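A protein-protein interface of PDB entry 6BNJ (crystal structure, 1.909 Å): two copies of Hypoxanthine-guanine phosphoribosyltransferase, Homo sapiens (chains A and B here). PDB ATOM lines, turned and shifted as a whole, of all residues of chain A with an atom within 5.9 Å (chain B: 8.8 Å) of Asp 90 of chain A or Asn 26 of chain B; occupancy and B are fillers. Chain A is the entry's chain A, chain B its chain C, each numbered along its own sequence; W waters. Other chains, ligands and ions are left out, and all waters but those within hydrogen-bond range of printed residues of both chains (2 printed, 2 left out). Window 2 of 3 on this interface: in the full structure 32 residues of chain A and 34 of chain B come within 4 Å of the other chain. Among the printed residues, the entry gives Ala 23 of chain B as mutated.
Printed residues of chain B that touch a printed residue of chain A: Ala 23, Ile 24, Pro 25, Asn 26 and His 27. Hydrophobic or aromatic side chains of chain B within 4 Å of the printed part of chain A: Ala 23 and His 27. Among the printed residues, no Asp or Glu carboxylate lies within 4 Å of a Lys or Arg side-chain nitrogen of the other chain.
Printed residues of chain A within 4 Å of Asn 26 of chain B: Asn 86 (3.7 Å), Ser 89 (3.9 Å), Asp 90 (2.7 Å) and Ser 92 (3.3 Å). Of the printed residues of chain B, Ser 92 of chain A touches Asn 26 (3.3 Å) and His 27 (2.9 Å). Of the printed residues of chain A, His 27 of chain B touches Ser 92. Of the printed residues of chain A, Ala 23 of chain B touches Arg 87 (3.6 Å) and Asn 88 (3.9 Å). Printed residues of chain B within 4 Å of Asn 88 of chain A: Ala 23. Glu 30 of chain B touches none of the printed residues of chain A. The nearest printed residue of chain B that does not touch Asn 86 of chain A is His 27 of chain B (4.3 Å).
A ring nitrogen (NE2) of His 27 of chain B sits at hydrogen-bond distance from the side-chain carboxylate (OD2) of Asp 201 of chain B, 3.0 Å away.
The side-chain amide nitrogen (ND2) of Asn 26 of chain B lies within hydrogen-bond range of the backbone carbonyl oxygen (O) of Asp 90 of chain A (2.7 Å). ND1 of His 27 of chain B sits at hydrogen-bond distance from OG of Ser 92 of chain A.
Among the printed residues, pairs that only touch across the chains: Asn 86 of chain A with Pro 25 of chain B (3.5 Å), Asn 86 of chain A with Asn 26 of chain B (3.7 Å), Arg 87 of chain A with Ala 23 of chain B (3.6 Å), Arg 87 of chain A with Ile 24 of chain B (3.6 Å), Arg 87 of chain A with Pro 25 of chain B (3.6 Å), Asn 88 of chain A with Ala 23 of chain B (3.9 Å), Ser 89 of chain A with Asn 26 of chain B (3.9 Å) and Ser 92 of chain A with Asn 26 of chain B (3.3 Å).
No position is printed for both chains.
Water W1 lies within hydrogen-bond range of ND2 of Asn 86 of chain A (2.5 Å) and OD2 of Asp 201 of chain B (2.8 Å). Water W2 bridges the backbone carbonyl oxygen of Asp 201 of chain B and the side-chain amide nitrogen of Asn 86 of chain A.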
ATOM      1  N   ASN A  86      26.268 -18.046   8.924  1.00  0.00           N
ATOM      2  CA  ASN A  86      26.502 -19.169   9.821  1.00  0.00           C
ATOM      3  C   ASN A  86      27.502 -20.225   9.323  1.00  0.00           C
ATOM      4  O   ASN A  86      28.044 -20.973  10.143  1.00  0.00           O
ATOM      5  CB  ASN A  86      25.170 -19.866  10.118  1.00  0.00           C
ATOM      6  CG  ASN A  86      24.268 -19.041  10.985  1.00  0.00           C
ATOM      7  OD1 ASN A  86      24.653 -17.987  11.486  1.00  0.00           O
ATOM      8  ND2 ASN A  86      23.055 -19.514  11.169  1.00  0.00           N
ATOM      9  N   ARG A  87      27.736 -20.329   8.015  1.00  0.00           N
ATOM     10  CA  ARG A  87      28.694 -21.349   7.550  1.00  0.00           C
ATOM     11  C   ARG A  87      30.023 -20.705   7.192  1.00  0.00           C
ATOM     12  O   ARG A  87      30.963 -21.393   6.819  1.00  0.00           O
ATOM     13  CB  ARG A  87      28.154 -22.154   6.345  1.00  0.00           C
ATOM     14  CG  ARG A  87      27.871 -21.288   5.101  1.00  0.00           C
ATOM     15  CD  ARG A  87      27.308 -22.115   3.946  1.00  0.00           C
ATOM     16  NE  ARG A  87      27.128 -21.233   2.795  1.00  0.00           N
ATOM     17  CZ  ARG A  87      25.951 -20.762   2.443  1.00  0.00           C
ATOM     18  NH1 ARG A  87      24.879 -21.147   3.126  1.00  0.00           N
ATOM     19  NH2 ARG A  87      25.843 -19.919   1.407  1.00  0.00           N
ATOM     20  N   ASN A  88      30.132 -19.389   7.337  1.00  0.00           N
ATOM     21  CA  ASN A  88      31.407 -18.743   7.074  1.00  0.00           C
ATOM     22  C   ASN A  88      31.996 -18.011   8.280  1.00  0.00           C
ATOM     23  O   ASN A  88      32.944 -17.245   8.147  1.00  0.00           O
ATOM     24  CB  ASN A  88      31.272 -17.778   5.884  1.00  0.00           C
ATOM     25  CG  ASN A  88      31.129 -18.518   4.549  1.00  0.00           C
ATOM     26  OD1 ASN A  88      32.046 -19.236   4.126  1.00  0.00           O
ATOM     27  ND2 ASN A  88      29.985 -18.362   3.891  1.00  0.00           N
ATOM     28  N   SER A  89      31.438 -18.265   9.456  1.00  0.00           N
ATOM     29  CA  SER A  89      31.922 -17.682  10.693  1.00  0.00           C
ATOM     30  C   SER A  89      32.272 -18.746  11.726  1.00  0.00           C
ATOM     31  O   SER A  89      31.878 -19.912  11.606  1.00  0.00           O
ATOM     32  CB  SER A  89      30.875 -16.735  11.301  1.00  0.00           C
ATOM     33  OG  SER A  89      30.615 -15.608  10.476  1.00  0.00           O
ATOM     34  N   ASP A  90      33.028 -18.307  12.726  1.00  0.00           N
ATOM     35  CA  ASP A  90      33.267 -19.101  13.921  1.00  0.00           C
ATOM     36  C   ASP A  90      31.991 -19.144  14.755  1.00  0.00           C
ATOM     37  O   ASP A  90      31.692 -20.158  15.386  1.00  0.00           O
ATOM     38  CB  ASP A  90      34.416 -18.522  14.759  1.00  0.00           C
ATOM     39  CG  ASP A  90      35.703 -18.351  13.970  1.00  0.00           C
ATOM     40  OD1 ASP A  90      35.938 -19.109  13.005  1.00  0.00           O
ATOM     41  OD2 ASP A  90      36.489 -17.450  14.327  1.00  0.00           O
ATOM     42  N   ARG A  91      31.244 -18.036  14.747  1.00  0.00           N
ATOM     43  CA  ARG A  91      30.006 -17.938  15.517  1.00  0.00           C
ATOM     44  C   ARG A  91      28.814 -18.383  14.664  1.00  0.00           C
ATOM     45  O   ARG A  91      28.604 -17.902  13.533  1.00  0.00           O
ATOM     46  CB  ARG A  91      29.810 -16.506  16.088  1.00  0.00           C
ATOM     47  CG  ARG A  91      29.198 -15.429  15.151  1.00  0.00           C
ATOM     48  CD  ARG A  91      30.068 -14.159  15.145  1.00  0.00           C
ATOM     49  NE  ARG A  91      29.334 -12.884  15.080  1.00  0.00           N
ATOM     50  CZ  ARG A  91      29.784 -11.802  14.432  1.00  0.00           C
ATOM     51  NH1 ARG A  91      30.940 -11.860  13.773  1.00  0.00           N
ATOM     52  NH2 ARG A  91      29.080 -10.670  14.424  1.00  0.00           N
ATOM     53  N   SER A  92      28.092 -19.371  15.199  1.00  0.00           N
ATOM     54  CA  SER A  92      26.886 -19.897  14.557  1.00  0.00           C
ATOM     55  C   SER A  92      25.954 -20.449  15.620  1.00  0.00           C
ATOM     56  O   SER A  92      26.354 -20.696  16.758  1.00  0.00           O
ATOM     57  CB  SER A  92      27.212 -20.986  13.518  1.00  0.00           C
ATOM     58  OG  SER A  92      27.303 -22.280  14.103  1.00  0.00           O
ATOM     59  N   ALA B  23      31.842 -25.343   2.927  1.00  0.00           N
ATOM     60  CA  ALA B  23      31.493 -24.445   4.016  1.00  0.00           C
ATOM     61  C   ALA B  23      30.241 -25.013   4.691  1.00  0.00           C
ATOM     62  O   ALA B  23      29.221 -25.206   4.040  1.00  0.00           O
ATOM     63  CB  ALA B  23      31.228 -23.008   3.479  1.00  0.00           C
ATOM     64  N   ILE B  24      30.364 -25.325   5.973  1.00  0.00           N
ATOM     65  CA  ILE B  24      29.356 -26.053   6.735  1.00  0.00           C
ATOM     66  C   ILE B  24      29.049 -25.268   8.015  1.00  0.00           C
ATOM     67  O   ILE B  24      29.969 -24.912   8.711  1.00  0.00           O
ATOM     68  CB  ILE B  24      29.909 -27.464   7.137  1.00  0.00           C
ATOM     69  CG1 ILE B  24      30.278 -28.278   5.882  1.00  0.00           C
ATOM     70  CG2 ILE B  24      28.993 -28.173   8.122  1.00  0.00           C
ATOM     71  CD1 ILE B  24      29.113 -28.616   4.973  1.00  0.00           C
ATOM     72  N   PRO B  25      27.779 -25.061   8.349  1.00  0.00           N
ATOM     73  CA  PRO B  25      27.522 -24.399   9.646  1.00  0.00           C
ATOM     74  C   PRO B  25      28.266 -25.037  10.832  1.00  0.00           C
ATOM     75  O   PRO B  25      28.161 -26.263  10.991  1.00  0.00           O
ATOM     76  CB  PRO B  25      26.010 -24.554   9.831  1.00  0.00           C
ATOM     77  CG  PRO B  25      25.481 -25.131   8.621  1.00  0.00           C
ATOM     78  CD  PRO B  25      26.584 -25.706   7.795  1.00  0.00           C
ATOM     79  N   ASN B  26      28.990 -24.247  11.649  1.00  0.00           N
ATOM     80  CA  ASN B  26      29.729 -24.770  12.815  1.00  0.00           C
ATOM     81  C   ASN B  26      28.892 -25.623  13.718  1.00  0.00           C
ATOM     82  O   ASN B  26      29.390 -26.581  14.279  1.00  0.00           O
ATOM     83  CB  ASN B  26      30.284 -23.656  13.719  1.00  0.00           C
ATOM     84  CG  ASN B  26      31.731 -23.345  13.466  1.00  0.00           C
ATOM     85  OD1 ASN B  26      32.284 -23.696  12.417  1.00  0.00           O
ATOM     86  ND2 ASN B  26      32.358 -22.640  14.416  1.00  0.00           N
ATOM     87  N   HIS B  27      27.635 -25.225  13.920  1.00  0.00           N
ATOM     88  CA  HIS B  27      26.820 -25.924  14.893  1.00  0.00           C
ATOM     89  C   HIS B  27      26.385 -27.309  14.397  1.00  0.00           C
ATOM     90  O   HIS B  27      25.845 -28.073  15.169  1.00  0.00           O
ATOM     91  CB  HIS B  27      25.614 -25.079  15.278  1.00  0.00           C
ATOM     92  CG  HIS B  27      24.703 -24.740  14.144  1.00  0.00           C
ATOM     93  ND1 HIS B  27      24.873 -23.616  13.353  1.00  0.00           N
ATOM     94  CD2 HIS B  27      23.560 -25.325  13.713  1.00  0.00           C
ATOM     95  CE1 HIS B  27      23.898 -23.550  12.465  1.00  0.00           C
ATOM     96  NE2 HIS B  27      23.079 -24.574  12.669  1.00  0.00           N
ATOM     97  N   TYR B  28      26.625 -27.636  13.127  1.00  0.00           N
ATOM     98  CA  TYR B  28      26.359 -29.006  12.663  1.00  0.00           C
ATOM     99  C   TYR B  28      27.658 -29.794  12.374  1.00  0.00           C
ATOM    100  O   TYR B  28      27.618 -30.899  11.799  1.00  0.00           O
ATOM    101  CB  TYR B  28      25.466 -28.987  11.411  1.00  0.00           C
ATOM    102  CG  TYR B  28      24.036 -28.560  11.674  1.00  0.00           C
ATOM    103  CD1 TYR B  28      23.366 -28.942  12.839  1.00  0.00           C
ATOM    104  CD2 TYR B  28      23.345 -27.744  10.746  1.00  0.00           C
ATOM    105  CE1 TYR B  28      22.049 -28.542  13.071  1.00  0.00           C
ATOM    106  CE2 TYR B  28      22.041 -27.339  10.977  1.00  0.00           C
ATOM    107  CZ  TYR B  28      21.388 -27.739  12.117  1.00  0.00           C
ATOM    108  OH  TYR B  28      20.082 -27.315  12.339  1.00  0.00           O
ATOM    109  N   ALA B  29      28.801 -29.221  12.767  1.00  0.00           N
ATOM    110  CA  ALA B  29      30.102 -29.774  12.380  1.00  0.00           C
ATOM    111  C   ALA B  29      30.284 -31.230  12.826  1.00  0.00           C
ATOM    112  O   ALA B  29      30.804 -32.060  12.085  1.00  0.00           O
ATOM    113  CB  ALA B  29      31.257 -28.912  12.949  1.00  0.00           C
ATOM    114  N   GLU B  30      29.875 -31.540  14.047  1.00  0.00           N
ATOM    115  CA  GLU B  30      29.986 -32.883  14.600  1.00  0.00           C
ATOM    116  C   GLU B  30      28.804 -33.767  14.195  1.00  0.00           C
ATOM    117  O   GLU B  30      28.838 -34.974  14.373  1.00  0.00           O
ATOM    118  CB  GLU B  30      30.077 -32.828  16.139  1.00  0.00           C
ATOM    119  CG  GLU B  30      31.354 -32.158  16.692  1.00  0.00           C
ATOM    120  CD  GLU B  30      31.312 -31.896  18.199  1.00  0.00           C
ATOM    121  OE1 GLU B  30      32.296 -32.226  18.883  1.00  0.00           O
ATOM    122  OE2 GLU B  30      30.306 -31.348  18.700  1.00  0.00           O
ATOM    123  N   ASP B  31      27.742 -33.156  13.656  1.00  0.00           N
ATOM    124  CA  ASP B  31      26.443 -33.831  13.479  1.00  0.00           C
ATOM    125  C   ASP B  31      26.166 -34.430  12.106  1.00  0.00           C
ATOM    126  O   ASP B  31      25.157 -35.136  11.912  1.00  0.00           O
ATOM    127  CB  ASP B  31      25.308 -32.844  13.825  1.00  0.00           C
ATOM    128  CG  ASP B  31      25.465 -32.256  15.216  1.00  0.00           C
ATOM    129  OD1 ASP B  31      25.773 -33.027  16.140  1.00  0.00           O
ATOM    130  OD2 ASP B  31      25.322 -31.023  15.392  1.00  0.00           O
ATOM    131  N   LEU B  32      27.029 -34.134  11.149  1.00  0.00           N
ATOM    132  CA  LEU B  32      26.854 -34.594   9.760  1.00  0.00           C
ATOM    133  C   LEU B  32      27.964 -35.546   9.423  1.00  0.00           C
ATOM    134  O   LEU B  32      29.038 -35.456  10.013  1.00  0.00           O
ATOM    135  CB  LEU B  32      26.882 -33.433   8.784  1.00  0.00           C
ATOM    136  CG  LEU B  32      25.761 -32.426   8.967  1.00  0.00           C
ATOM    137  CD1 LEU B  32      25.974 -31.276   8.001  1.00  0.00           C
ATOM    138  CD2 LEU B  32      24.415 -33.095   8.731  1.00  0.00           C
ATOM    139  N   ASP B 201      18.147 -25.541   8.229  1.00  0.00           N
ATOM    140  CA  ASP B 201      19.043 -24.375   8.058  1.00  0.00           C
ATOM    141  C   ASP B 201      20.414 -24.825   7.558  1.00  0.00           C
ATOM    142  O   ASP B 201      21.444 -24.488   8.131  1.00  0.00           O
ATOM    143  CB  ASP B 201      19.196 -23.602   9.378  1.00  0.00           C
ATOM    144  CG  ASP B 201      19.720 -24.483  10.523  1.00  0.00           C
ATOM    145  OD1 ASP B 201      19.403 -25.698  10.515  1.00  0.00           O
ATOM    146  OD2 ASP B 201      20.439 -23.971  11.411  1.00  0.00           O
ATOM    147  N   LEU B 202      20.402 -25.584   6.474  1.00  0.00           N
ATOM    148  CA  LEU B 202      21.609 -26.183   5.870  1.00  0.00           C
ATOM    149  C   LEU B 202      21.379 -26.153   4.357  1.00  0.00           C
ATOM    150  O   LEU B 202      20.309 -26.630   3.930  1.00  0.00           O
ATOM    151  CB  LEU B 202      21.784 -27.619   6.378  1.00  0.00           C
ATOM    152  CG  LEU B 202      22.798 -28.567   5.723  1.00  0.00           C
ATOM    153  CD1 LEU B 202      24.226 -27.950   5.747  1.00  0.00           C
ATOM    154  CD2 LEU B 202      22.794 -29.957   6.394  1.00  0.00           C
ATOM    155  N   LYS B 215      22.034 -36.793  19.286  1.00  0.00           N
ATOM    156  CA  LYS B 215      21.895 -35.456  19.838  1.00  0.00           C
ATOM    157  C   LYS B 215      20.476 -34.918  19.633  1.00  0.00           C
ATOM    158  O   LYS B 215      19.902 -34.297  20.524  1.00  0.00           O
ATOM    159  CB  LYS B 215      22.926 -34.513  19.190  1.00  0.00           C
ATOM    160  CG  LYS B 215      22.891 -33.057  19.703  1.00  0.00           C
ATOM    161  CD  LYS B 215      23.948 -32.188  19.006  1.00  0.00           C
ATOM    162  CE  LYS B 215      25.380 -32.700  19.234  1.00  0.00           C
ATOM    163  NZ  LYS B 215      26.427 -32.000  18.370  1.00  0.00           N
ATOM    164  N   TYR B 216      19.917 -35.158  18.448  1.00  0.00           N
ATOM    165  CA  TYR B 216      18.662 -34.505  18.062  1.00  0.00           C
ATOM    166  C   TYR B 216      17.472 -35.471  18.086  1.00  0.00           C
ATOM    167  O   TYR B 216      16.369 -35.108  17.684  1.00  0.00           O
ATOM    168  CB  TYR B 216      18.779 -33.842  16.682  1.00  0.00           C
ATOM    169  CG  TYR B 216      19.834 -32.752  16.606  1.00  0.00           C
ATOM    170  CD1 TYR B 216      19.780 -31.630  17.425  1.00  0.00           C
ATOM    171  CD2 TYR B 216      20.905 -32.863  15.741  1.00  0.00           C
ATOM    172  CE1 TYR B 216      20.776 -30.634  17.376  1.00  0.00           C
ATOM    173  CE2 TYR B 216      21.901 -31.884  15.684  1.00  0.00           C
ATOM    174  CZ  TYR B 216      21.827 -30.769  16.504  1.00  0.00           C
ATOM    175  OH  TYR B 216      22.811 -29.802  16.427  1.00  0.00           O
HETATM  176  O   HOH W   1      21.498 -21.448  11.688  1.00  0.00           O
HETATM  177  O   HOH W   2      23.058 -22.464   9.386  1.00  0.00           O
